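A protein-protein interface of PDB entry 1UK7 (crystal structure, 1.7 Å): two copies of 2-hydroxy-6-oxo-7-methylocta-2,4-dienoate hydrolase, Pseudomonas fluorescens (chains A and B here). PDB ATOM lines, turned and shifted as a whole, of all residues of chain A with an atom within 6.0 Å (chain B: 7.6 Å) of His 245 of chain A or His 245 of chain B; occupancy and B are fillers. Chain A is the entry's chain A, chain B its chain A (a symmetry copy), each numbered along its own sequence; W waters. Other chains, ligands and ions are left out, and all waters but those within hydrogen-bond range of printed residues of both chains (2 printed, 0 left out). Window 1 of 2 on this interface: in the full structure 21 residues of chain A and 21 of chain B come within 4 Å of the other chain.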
ATOM      1  N   LEU A 217     -11.569  14.204  11.347  1.00  0.00           N
ATOM      2  CA  LEU A 217     -11.467  15.656  11.396  1.00  0.00           C
ATOM      3  C   LEU A 217     -12.643  16.196  10.586  1.00  0.00           C
ATOM      4  O   LEU A 217     -12.724  15.978   9.379  1.00  0.00           O
ATOM      5  CB  LEU A 217     -10.141  16.123  10.784  1.00  0.00           C
ATOM      6  CG  LEU A 217      -9.973  17.636  10.591  1.00  0.00           C
ATOM      7  CD1 LEU A 217     -10.096  18.369  11.924  1.00  0.00           C
ATOM      8  CD2 LEU A 217      -8.615  17.911   9.954  1.00  0.00           C
ATOM      9  N   ILE A 218     -13.556  16.882  11.264  1.00  0.00           N
ATOM     10  CA  ILE A 218     -14.748  17.449  10.638  1.00  0.00           C
ATOM     11  C   ILE A 218     -14.492  18.938  10.408  1.00  0.00           C
ATOM     12  O   ILE A 218     -14.147  19.664  11.339  1.00  0.00           O
ATOM     13  CB  ILE A 218     -15.969  17.261  11.566  1.00  0.00           C
ATOM     14  CG1 ILE A 218     -16.109  15.776  11.931  1.00  0.00           C
ATOM     15  CG2 ILE A 218     -17.237  17.773  10.892  1.00  0.00           C
ATOM     16  CD1 ILE A 218     -17.131  15.501  13.026  1.00  0.00           C
ATOM     17  N   ILE A 219     -14.651  19.379   9.163  1.00  0.00           N
ATOM     18  CA  ILE A 219     -14.415  20.770   8.795  1.00  0.00           C
ATOM     19  C   ILE A 219     -15.686  21.379   8.215  1.00  0.00           C
ATOM     20  O   ILE A 219     -16.388  20.735   7.440  1.00  0.00           O
ATOM     21  CB  ILE A 219     -13.276  20.860   7.755  1.00  0.00           C
ATOM     22  CG1 ILE A 219     -12.004  20.230   8.332  1.00  0.00           C
ATOM     23  CG2 ILE A 219     -13.037  22.315   7.362  1.00  0.00           C
ATOM     24  CD1 ILE A 219     -10.841  20.200   7.369  1.00  0.00           C
ATOM     25  N   HIS A 220     -15.978  22.621   8.587  1.00  0.00           N
ATOM     26  CA  HIS A 220     -17.189  23.277   8.106  1.00  0.00           C
ATOM     27  C   HIS A 220     -17.022  24.792   8.068  1.00  0.00           C
ATOM     28  O   HIS A 220     -16.295  25.367   8.875  1.00  0.00           O
ATOM     29  CB  HIS A 220     -18.371  22.916   9.023  1.00  0.00           C
ATOM     30  CG  HIS A 220     -19.696  22.857   8.323  1.00  0.00           C
ATOM     31  ND1 HIS A 220     -20.342  21.669   8.051  1.00  0.00           N
ATOM     32  CD2 HIS A 220     -20.487  23.836   7.821  1.00  0.00           C
ATOM     33  CE1 HIS A 220     -21.472  21.919   7.413  1.00  0.00           C
ATOM     34  NE2 HIS A 220     -21.584  23.226   7.260  1.00  0.00           N
ATOM     35  N   GLY A 221     -17.686  25.428   7.111  1.00  0.00           N
ATOM     36  CA  GLY A 221     -17.631  26.876   7.016  1.00  0.00           C
ATOM     37  C   GLY A 221     -18.826  27.414   7.780  1.00  0.00           C
ATOM     38  O   GLY A 221     -19.948  26.956   7.571  1.00  0.00           O
ATOM     39  N   GLN A 243     -12.661  15.611  15.793  1.00  0.00           N
ATOM     40  CA  GLN A 243     -12.233  16.977  16.042  1.00  0.00           C
ATOM     41  C   GLN A 243     -13.091  17.775  15.075  1.00  0.00           C
ATOM     42  O   GLN A 243     -13.387  17.306  13.975  1.00  0.00           O
ATOM     43  CB  GLN A 243     -10.768  17.192  15.674  1.00  0.00           C
ATOM     44  CG  GLN A 243      -9.771  16.524  16.591  1.00  0.00           C
ATOM     45  CD  GLN A 243      -8.347  16.826  16.181  1.00  0.00           C
ATOM     46  OE1 GLN A 243      -7.843  17.932  16.380  1.00  0.00           O
ATOM     47  NE2 GLN A 243      -7.690  15.840  15.591  1.00  0.00           N
ATOM     48  N   LEU A 244     -13.506  18.964  15.483  1.00  0.00           N
ATOM     49  CA  LEU A 244     -14.306  19.804  14.608  1.00  0.00           C
ATOM     50  C   LEU A 244     -13.583  21.121  14.429  1.00  0.00           C
ATOM     51  O   LEU A 244     -13.137  21.721  15.402  1.00  0.00           O
ATOM     52  CB  LEU A 244     -15.684  20.075  15.219  1.00  0.00           C
ATOM     53  CG  LEU A 244     -16.531  21.153  14.528  1.00  0.00           C
ATOM     54  CD1 LEU A 244     -17.026  20.644  13.164  1.00  0.00           C
ATOM     55  CD2 LEU A 244     -17.707  21.521  15.421  1.00  0.00           C
ATOM     56  N   HIS A 245     -13.443  21.557  13.183  1.00  0.00           N
ATOM     57  CA  HIS A 245     -12.817  22.838  12.935  1.00  0.00           C
ATOM     58  C   HIS A 245     -13.776  23.630  12.071  1.00  0.00           C
ATOM     59  O   HIS A 245     -14.091  23.228  10.945  1.00  0.00           O
ATOM     60  CB  HIS A 245     -11.485  22.705  12.205  1.00  0.00           C
ATOM     61  CG  HIS A 245     -10.652  23.949  12.278  1.00  0.00           C
ATOM     62  ND1 HIS A 245      -9.732  24.165  13.279  1.00  0.00           N
ATOM     63  CD2 HIS A 245     -10.649  25.068  11.514  1.00  0.00           C
ATOM     64  CE1 HIS A 245      -9.195  25.364  13.130  1.00  0.00           C
ATOM     65  NE2 HIS A 245      -9.734  25.932  12.067  1.00  0.00           N
ATOM     66  N   VAL A 246     -14.251  24.746  12.610  1.00  0.00           N
ATOM     67  CA  VAL A 246     -15.175  25.605  11.885  1.00  0.00           C
ATOM     68  C   VAL A 246     -14.476  26.902  11.487  1.00  0.00           C
ATOM     69  O   VAL A 246     -13.891  27.587  12.332  1.00  0.00           O
ATOM     70  CB  VAL A 246     -16.400  25.960  12.747  1.00  0.00           C
ATOM     71  CG1 VAL A 246     -17.386  26.790  11.932  1.00  0.00           C
ATOM     72  CG2 VAL A 246     -17.064  24.690  13.245  1.00  0.00           C
ATOM     73  N   PHE A 247     -14.538  27.223  10.197  1.00  0.00           N
ATOM     74  CA  PHE A 247     -13.932  28.444   9.678  1.00  0.00           C
ATOM     75  C   PHE A 247     -14.957  29.566   9.572  1.00  0.00           C
ATOM     76  O   PHE A 247     -15.967  29.421   8.890  1.00  0.00           O
ATOM     77  CB  PHE A 247     -13.351  28.210   8.278  1.00  0.00           C
ATOM     78  CG  PHE A 247     -12.136  27.330   8.252  1.00  0.00           C
ATOM     79  CD1 PHE A 247     -10.952  27.730   8.865  1.00  0.00           C
ATOM     80  CD2 PHE A 247     -12.160  26.122   7.568  1.00  0.00           C
ATOM     81  CE1 PHE A 247      -9.806  26.938   8.791  1.00  0.00           C
ATOM     82  CE2 PHE A 247     -11.023  25.322   7.486  1.00  0.00           C
ATOM     83  CZ  PHE A 247      -9.842  25.729   8.098  1.00  0.00           C
ATOM     84  N   LEU A 265      -4.111  21.992   8.220  1.00  0.00           N
ATOM     85  CA  LEU A 265      -4.883  21.171   9.147  1.00  0.00           C
ATOM     86  C   LEU A 265      -4.912  19.715   8.714  1.00  0.00           C
ATOM     87  O   LEU A 265      -4.683  18.814   9.520  1.00  0.00           O
ATOM     88  CB  LEU A 265      -6.320  21.685   9.247  1.00  0.00           C
ATOM     89  CG  LEU A 265      -6.592  22.870  10.172  1.00  0.00           C
ATOM     90  CD1 LEU A 265      -8.018  23.359   9.972  1.00  0.00           C
ATOM     91  CD2 LEU A 265      -6.368  22.446  11.624  1.00  0.00           C
ATOM     92  N   LEU B 125      -8.941  31.643  22.658  1.00  0.00           N
ATOM     93  CA  LEU B 125      -9.837  31.532  23.800  1.00  0.00           C
ATOM     94  C   LEU B 125     -10.149  30.060  24.029  1.00  0.00           C
ATOM     95  O   LEU B 125     -10.762  29.421  23.178  1.00  0.00           O
ATOM     96  CB  LEU B 125     -11.118  32.315  23.510  1.00  0.00           C
ATOM     97  CG  LEU B 125     -10.885  33.765  23.067  1.00  0.00           C
ATOM     98  CD1 LEU B 125     -12.205  34.394  22.624  1.00  0.00           C
ATOM     99  CD2 LEU B 125     -10.263  34.557  24.209  1.00  0.00           C
ATOM    100  N   LEU B 217      -9.033  32.415  17.612  1.00  0.00           N
ATOM    101  CA  LEU B 217      -9.094  30.962  17.551  1.00  0.00           C
ATOM    102  C   LEU B 217      -9.741  30.505  18.857  1.00  0.00           C
ATOM    103  O   LEU B 217      -9.182  30.701  19.934  1.00  0.00           O
ATOM    104  CB  LEU B 217      -7.685  30.370  17.420  1.00  0.00           C
ATOM    105  CG  LEU B 217      -7.572  28.844  17.536  1.00  0.00           C
ATOM    106  CD1 LEU B 217      -8.414  28.155  16.465  1.00  0.00           C
ATOM    107  CD2 LEU B 217      -6.107  28.439  17.405  1.00  0.00           C
ATOM    108  N   ILE B 218     -10.926  29.914  18.749  1.00  0.00           N
ATOM    109  CA  ILE B 218     -11.681  29.436  19.904  1.00  0.00           C
ATOM    110  C   ILE B 218     -11.471  27.926  20.008  1.00  0.00           C
ATOM    111  O   ILE B 218     -11.707  27.196  19.047  1.00  0.00           O
ATOM    112  CB  ILE B 218     -13.182  29.749  19.716  1.00  0.00           C
ATOM    113  CG1 ILE B 218     -13.361  31.248  19.438  1.00  0.00           C
ATOM    114  CG2 ILE B 218     -13.974  29.331  20.951  1.00  0.00           C
ATOM    115  CD1 ILE B 218     -14.768  31.635  19.004  1.00  0.00           C
ATOM    116  N   ILE B 219     -11.016  27.472  21.173  1.00  0.00           N
ATOM    117  CA  ILE B 219     -10.745  26.058  21.402  1.00  0.00           C
ATOM    118  C   ILE B 219     -11.595  25.546  22.559  1.00  0.00           C
ATOM    119  O   ILE B 219     -11.752  26.228  23.568  1.00  0.00           O
ATOM    120  CB  ILE B 219      -9.249  25.847  21.726  1.00  0.00           C
ATOM    121  CG1 ILE B 219      -8.395  26.380  20.571  1.00  0.00           C
ATOM    122  CG2 ILE B 219      -8.969  24.369  21.978  1.00  0.00           C
ATOM    123  CD1 ILE B 219      -6.908  26.289  20.813  1.00  0.00           C
ATOM    124  N   HIS B 220     -12.140  24.342  22.415  1.00  0.00           N
ATOM    125  CA  HIS B 220     -12.992  23.780  23.457  1.00  0.00           C
ATOM    126  C   HIS B 220     -12.958  22.256  23.441  1.00  0.00           C
ATOM    127  O   HIS B 220     -12.791  21.640  22.391  1.00  0.00           O
ATOM    128  CB  HIS B 220     -14.440  24.261  23.255  1.00  0.00           C
ATOM    129  CG  HIS B 220     -15.219  24.416  24.527  1.00  0.00           C
ATOM    130  ND1 HIS B 220     -15.535  25.648  25.061  1.00  0.00           N
ATOM    131  CD2 HIS B 220     -15.727  23.496  25.383  1.00  0.00           C
ATOM    132  CE1 HIS B 220     -16.204  25.481  26.188  1.00  0.00           C
ATOM    133  NE2 HIS B 220     -16.334  24.184  26.406  1.00  0.00           N
ATOM    134  N   GLY B 221     -13.098  21.656  24.616  1.00  0.00           N
ATOM    135  CA  GLY B 221     -13.126  20.208  24.704  1.00  0.00           C
ATOM    136  C   GLY B 221     -14.584  19.791  24.661  1.00  0.00           C
ATOM    137  O   GLY B 221     -15.403  20.338  25.398  1.00  0.00           O
ATOM    138  N   ARG B 222     -14.919  18.829  23.808  1.00  0.00           N
ATOM    139  CA  ARG B 222     -16.304  18.382  23.681  1.00  0.00           C
ATOM    140  C   ARG B 222     -16.931  18.027  25.027  1.00  0.00           C
ATOM    141  O   ARG B 222     -18.063  18.408  25.320  1.00  0.00           O
ATOM    142  CB  ARG B 222     -16.380  17.166  22.751  1.00  0.00           C
ATOM    143  CG  ARG B 222     -17.787  16.628  22.546  1.00  0.00           C
ATOM    144  CD  ARG B 222     -17.792  15.510  21.516  1.00  0.00           C
ATOM    145  NE  ARG B 222     -17.009  14.363  21.956  1.00  0.00           N
ATOM    146  CZ  ARG B 222     -16.589  13.392  21.153  1.00  0.00           C
ATOM    147  NH1 ARG B 222     -16.868  13.426  19.857  1.00  0.00           N
ATOM    148  NH2 ARG B 222     -15.894  12.377  21.648  1.00  0.00           N
ATOM    149  N   LEU B 229     -19.735  23.540  25.974  1.00  0.00           N
ATOM    150  CA  LEU B 229     -19.313  23.778  24.596  1.00  0.00           C
ATOM    151  C   LEU B 229     -20.189  24.848  23.953  1.00  0.00           C
ATOM    152  O   LEU B 229     -19.722  25.654  23.139  1.00  0.00           O
ATOM    153  CB  LEU B 229     -19.411  22.482  23.784  1.00  0.00           C
ATOM    154  CG  LEU B 229     -19.245  22.616  22.267  1.00  0.00           C
ATOM    155  CD1 LEU B 229     -17.840  23.118  21.946  1.00  0.00           C
ATOM    156  CD2 LEU B 229     -19.495  21.267  21.605  1.00  0.00           C
ATOM    157  N   SER B 232     -18.781  28.333  23.739  1.00  0.00           N
ATOM    158  CA  SER B 232     -17.825  28.616  22.673  1.00  0.00           C
ATOM    159  C   SER B 232     -18.521  28.665  21.320  1.00  0.00           C
ATOM    160  O   SER B 232     -18.070  29.363  20.416  1.00  0.00           O
ATOM    161  CB  SER B 232     -16.700  27.580  22.663  1.00  0.00           C
ATOM    162  OG  SER B 232     -15.788  27.876  23.708  1.00  0.00           O
ATOM    163  N   ALA B 242     -13.392  34.532  13.445  1.00  0.00           N
ATOM    164  CA  ALA B 242     -13.179  33.442  14.373  1.00  0.00           C
ATOM    165  C   ALA B 242     -13.127  32.069  13.736  1.00  0.00           C
ATOM    166  O   ALA B 242     -13.757  31.804  12.713  1.00  0.00           O
ATOM    167  CB  ALA B 242     -14.268  33.457  15.436  1.00  0.00           C
ATOM    168  N   GLN B 243     -12.338  31.209  14.361  1.00  0.00           N
ATOM    169  CA  GLN B 243     -12.212  29.818  13.961  1.00  0.00           C
ATOM    170  C   GLN B 243     -12.528  29.073  15.248  1.00  0.00           C
ATOM    171  O   GLN B 243     -12.186  29.541  16.335  1.00  0.00           O
ATOM    172  CB  GLN B 243     -10.787  29.471  13.543  1.00  0.00           C
ATOM    173  CG  GLN B 243     -10.336  30.073  12.233  1.00  0.00           C
ATOM    174  CD  GLN B 243      -8.932  29.642  11.874  1.00  0.00           C
ATOM    175  OE1 GLN B 243      -8.695  28.501  11.473  1.00  0.00           O
ATOM    176  NE2 GLN B 243      -7.986  30.554  12.028  1.00  0.00           N
ATOM    177  N   LEU B 244     -13.191  27.934  15.133  1.00  0.00           N
ATOM    178  CA  LEU B 244     -13.507  27.145  16.311  1.00  0.00           C
ATOM    179  C   LEU B 244     -12.908  25.768  16.131  1.00  0.00           C
ATOM    180  O   LEU B 244     -13.068  25.154  15.080  1.00  0.00           O
ATOM    181  CB  LEU B 244     -15.023  27.006  16.487  1.00  0.00           C
ATOM    182  CG  LEU B 244     -15.492  25.988  17.536  1.00  0.00           C
ATOM    183  CD1 LEU B 244     -15.185  26.505  18.951  1.00  0.00           C
ATOM    184  CD2 LEU B 244     -16.984  25.742  17.368  1.00  0.00           C
ATOM    185  N   HIS B 245     -12.195  25.292  17.145  1.00  0.00           N
ATOM    186  CA  HIS B 245     -11.641  23.958  17.072  1.00  0.00           C
ATOM    187  C   HIS B 245     -12.094  23.230  18.320  1.00  0.00           C
ATOM    188  O   HIS B 245     -11.762  23.631  19.441  1.00  0.00           O
ATOM    189  CB  HIS B 245     -10.117  23.960  17.025  1.00  0.00           C
ATOM    190  CG  HIS B 245      -9.544  22.652  16.569  1.00  0.00           C
ATOM    191  ND1 HIS B 245      -9.278  22.382  15.246  1.00  0.00           N
ATOM    192  CD2 HIS B 245      -9.250  21.519  17.253  1.00  0.00           C
ATOM    193  CE1 HIS B 245      -8.844  21.138  15.131  1.00  0.00           C
ATOM    194  NE2 HIS B 245      -8.817  20.594  16.334  1.00  0.00           N
ATOM    195  N   VAL B 246     -12.870  22.172  18.121  1.00  0.00           N
ATOM    196  CA  VAL B 246     -13.371  21.377  19.233  1.00  0.00           C
ATOM    197  C   VAL B 246     -12.680  20.017  19.253  1.00  0.00           C
ATOM    198  O   VAL B 246     -12.662  19.304  18.244  1.00  0.00           O
ATOM    199  CB  VAL B 246     -14.888  21.147  19.117  1.00  0.00           C
ATOM    200  CG1 VAL B 246     -15.393  20.386  20.338  1.00  0.00           C
ATOM    201  CG2 VAL B 246     -15.602  22.480  18.994  1.00  0.00           C
ATOM    202  N   PHE B 247     -12.107  19.673  20.404  1.00  0.00           N
ATOM    203  CA  PHE B 247     -11.429  18.392  20.574  1.00  0.00           C
ATOM    204  C   PHE B 247     -12.351  17.359  21.209  1.00  0.00           C
ATOM    205  O   PHE B 247     -12.861  17.574  22.305  1.00  0.00           O
ATOM    206  CB  PHE B 247     -10.202  18.544  21.482  1.00  0.00           C
ATOM    207  CG  PHE B 247      -9.070  19.316  20.871  1.00  0.00           C
ATOM    208  CD1 PHE B 247      -8.398  18.832  19.753  1.00  0.00           C
ATOM    209  CD2 PHE B 247      -8.643  20.506  21.445  1.00  0.00           C
ATOM    210  CE1 PHE B 247      -7.309  19.522  19.219  1.00  0.00           C
ATOM    211  CE2 PHE B 247      -7.557  21.205  20.923  1.00  0.00           C
ATOM    212  CZ  PHE B 247      -6.887  20.714  19.807  1.00  0.00           C
ATOM    213  N   GLY B 248     -12.572  16.244  20.523  1.00  0.00           N
ATOM    214  CA  GLY B 248     -13.391  15.195  21.096  1.00  0.00           C
ATOM    215  C   GLY B 248     -12.492  14.482  22.088  1.00  0.00           C
ATOM    216  O   GLY B 248     -11.267  14.558  21.970  1.00  0.00           O
ATOM    217  N   THR B 254      -7.758  21.419  27.788  1.00  0.00           N
ATOM    218  CA  THR B 254      -7.317  21.262  26.401  1.00  0.00           C
ATOM    219  C   THR B 254      -5.807  21.347  26.172  1.00  0.00           C
ATOM    220  O   THR B 254      -5.258  20.571  25.391  1.00  0.00           O
ATOM    221  CB  THR B 254      -8.018  22.259  25.443  1.00  0.00           C
ATOM    222  OG1 THR B 254      -7.665  23.607  25.780  1.00  0.00           O
ATOM    223  CG2 THR B 254      -9.521  22.084  25.521  1.00  0.00           C
ATOM    224  N   GLN B 258      -4.634  17.543  25.224  1.00  0.00           N
ATOM    225  CA  GLN B 258      -4.438  17.511  23.768  1.00  0.00           C
ATOM    226  C   GLN B 258      -3.257  18.434  23.467  1.00  0.00           C
ATOM    227  O   GLN B 258      -3.260  19.195  22.494  1.00  0.00           O
ATOM    228  CB  GLN B 258      -5.692  18.017  23.042  1.00  0.00           C
ATOM    229  CG  GLN B 258      -6.928  17.161  23.256  1.00  0.00           C
ATOM    230  CD  GLN B 258      -6.902  15.880  22.445  1.00  0.00           C
ATOM    231  OE1 GLN B 258      -6.929  15.913  21.218  1.00  0.00           O
ATOM    232  NE2 GLN B 258      -6.853  14.746  23.128  1.00  0.00           N
ATOM    233  N   ARG B 261      -1.515  18.665  19.792  1.00  0.00           N
ATOM    234  CA  ARG B 261      -2.452  19.232  18.824  1.00  0.00           C
ATOM    235  C   ARG B 261      -2.681  20.712  19.128  1.00  0.00           C
ATOM    236  O   ARG B 261      -2.711  21.546  18.222  1.00  0.00           O
ATOM    237  CB  ARG B 261      -3.785  18.488  18.885  1.00  0.00           C
ATOM    238  CG  ARG B 261      -3.743  17.086  18.308  1.00  0.00           C
ATOM    239  CD  ARG B 261      -5.043  16.352  18.574  1.00  0.00           C
ATOM    240  NE  ARG B 261      -5.121  15.105  17.823  1.00  0.00           N
ATOM    241  CZ  ARG B 261      -6.134  14.252  17.905  1.00  0.00           C
ATOM    242  NH1 ARG B 261      -7.153  14.509  18.713  1.00  0.00           N
ATOM    243  NH2 ARG B 261      -6.142  13.158  17.153  1.00  0.00           N
ATOM    244  N   PHE B 262      -2.851  21.019  20.410  1.00  0.00           N
ATOM    245  CA  PHE B 262      -3.082  22.387  20.871  1.00  0.00           C
ATOM    246  C   PHE B 262      -1.915  23.297  20.496  1.00  0.00           C
ATOM    247  O   PHE B 262      -2.104  24.357  19.903  1.00  0.00           O
ATOM    248  CB  PHE B 262      -3.261  22.395  22.394  1.00  0.00           C
ATOM    249  CG  PHE B 262      -3.417  23.770  22.981  1.00  0.00           C
ATOM    250  CD1 PHE B 262      -4.664  24.379  23.034  1.00  0.00           C
ATOM    251  CD2 PHE B 262      -2.310  24.461  23.473  1.00  0.00           C
ATOM    252  CE1 PHE B 262      -4.814  25.655  23.568  1.00  0.00           C
ATOM    253  CE2 PHE B 262      -2.446  25.741  24.010  1.00  0.00           C
ATOM    254  CZ  PHE B 262      -3.700  26.339  24.059  1.00  0.00           C
ATOM    255  N   LEU B 265      -1.711  23.952  16.720  1.00  0.00           N
ATOM    256  CA  LEU B 265      -2.772  24.856  16.291  1.00  0.00           C
ATOM    257  C   LEU B 265      -2.455  26.300  16.645  1.00  0.00           C
ATOM    258  O   LEU B 265      -2.589  27.196  15.814  1.00  0.00           O
ATOM    259  CB  LEU B 265      -4.100  24.469  16.942  1.00  0.00           C
ATOM    260  CG  LEU B 265      -4.902  23.333  16.309  1.00  0.00           C
ATOM    261  CD1 LEU B 265      -6.067  22.963  17.214  1.00  0.00           C
ATOM    262  CD2 LEU B 265      -5.408  23.770  14.935  1.00  0.00           C
HETATM  263  O   HOH W   1      -5.839  19.675  14.770  1.00  0.00           O
HETATM  264  O   HOH W   2      -6.308  26.558  11.889  1.00  0.00           O
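Gln 243 of chain A touches Val 246 of chain B (CA to O, 3.2 Å).
Gln 243 of chain A touches Phe 247 of chain B.
CA of His 245 of chain B touches O of Leu 244 of chain A (3.2 Å).
His 245 of chain A touches Leu 244 of chain B (CA to O, 3.2 Å).
Val 246 of chain A touches Gln 243 of chain B.
Gln 243 of chain B touches Phe 247 of chain A.
CD2 of Leu 265 of chain B touches CD2 of Leu 265 of chain A, 3.7 Å away.
Of the 21 printed residues of chain B, 7 touch a printed residue of chain A.
Hydrophobic or aromatic side chains of chain A within 4 Å of the printed part of chain B: His 245, Phe 247 and Leu 265.
Among the printed residues, 14 pairs touch across the chains.
Among the printed residues, no Asp or Glu carboxylate lies within 4 Å of a Lys or Arg side-chain nitrogen of the other chain.
A ring nitrogen (ND1) of His 245 of chain A is in hydrogen-bond range of a ring nitrogen (ND1) of His 245 of chain B, at 2.7 Å.
O of Leu 244 of chain A lies close to O of Leu 244 of chain B (3.4 Å).
O of Leu 244 of chain A sits at hydrogen-bond distance from N of Val 246 of chain B (2.8 Å).
A ring nitrogen (NE2) of His 245 of chain A sits at hydrogen-bond distance from the side-chain amide oxygen (OE1) of Gln 243 of chain B (2.8 Å).
N of Val 246 of chain A is in hydrogen-bond range of O of Leu 244 of chain B (2.8 Å).
NE2 of His 245 of chain B sits at hydrogen-bond distance from OE1 of Gln 243 of chain A, 2.8 Å away.
NE2 of Gln 243 of chain A sits close to NH1 of Arg 261 of chain B, at 3.4 Å.
N of Ile 218 of chain A sits at hydrogen-bond distance from O of Gln 243 of chain A (2.7 Å).
The backbone carbonyl oxygen (O) of His 220 of chain B sits at hydrogen-bond distance from the backbone NH (N) of Phe 247 of chain B (2.9 Å).
The backbone carbonyl oxygen of Ile 218 of chain B sits at hydrogen-bond distance from the backbone NH of His 245 of chain B (2.7 Å).
O of Ile 218 of chain A is in hydrogen-bond range of N of His 245 of chain A (2.7 Å).
The backbone NH (N) of Ile 218 of chain B is in hydrogen-bond range of the backbone carbonyl oxygen (O) of Gln 243 of chain B.
The backbone NH (N) of His 220 of chain A is in hydrogen-bond range of the backbone carbonyl oxygen (O) of His 245 of chain A (3.1 Å).
His 245 of chain A touches just these residues of chain B: Gln 243, Leu 244 and His 245.
Printed residues of chain B within 4 Å of Val 246 of chain A: Gln 243 (3.2 Å) and Leu 244 (2.8 Å).
Printed residues of chain B within 4 Å of Phe 247 of chain A: Gln 243.
Leu 217 of chain B touches none of the printed residues of chain A.
Printed residues of chain A within 4 Å of Leu 244 of chain B: Leu 244, His 245 and Val 246.
Printed residues of chain A within 4 Å of Val 246 of chain B: Gln 243 (3.2 Å) and Leu 244 (2.8 Å).
Of the printed residues of chain A, Leu 265 of chain B touches Leu 265 (3.7 Å).
The nearest printed residue of chain B that does not touch Gln 243 of chain A is Gly 248 of chain B (4.6 Å).
Water W2 lies within hydrogen-bond range of the side-chain amide oxygen (OE1) of Gln 243 of chain B (3.1 Å) and a ring nitrogen (NE2) of His 245 of chain A (3.5 Å).
Water W1 lies within hydrogen-bond range of the side-chain amide oxygen (OE1) of Gln 243 of chain A (3.1 Å) and a ring nitrogen (NE2) of His 245 of chain B (3.5 Å).
Gln 243 of chain A touches Val 246 of chain B, and with the chains exchanged Val 246 of chain A touches Gln 243 of chain B.
Gln 243 of chain A touches Phe 247 of chain B, and with the chains exchanged Phe 247 of chain A touches Gln 243 of chain B.
Leu 244 of chain B touches its own counterpart, Leu 244 of chain A.
Leu 244 of chain A touches Val 246 of chain B, and with the chains exchanged Val 246 of chain A touches Leu 244 of chain B.
Positions printed for both chains: 217, 218, 219, 220, 221, 243, 244, 245, 246, 247 and 265.
Of the 14 pairs that touch across the chains among the printed residues, 13 have their exchanged pair printed and touching as well.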
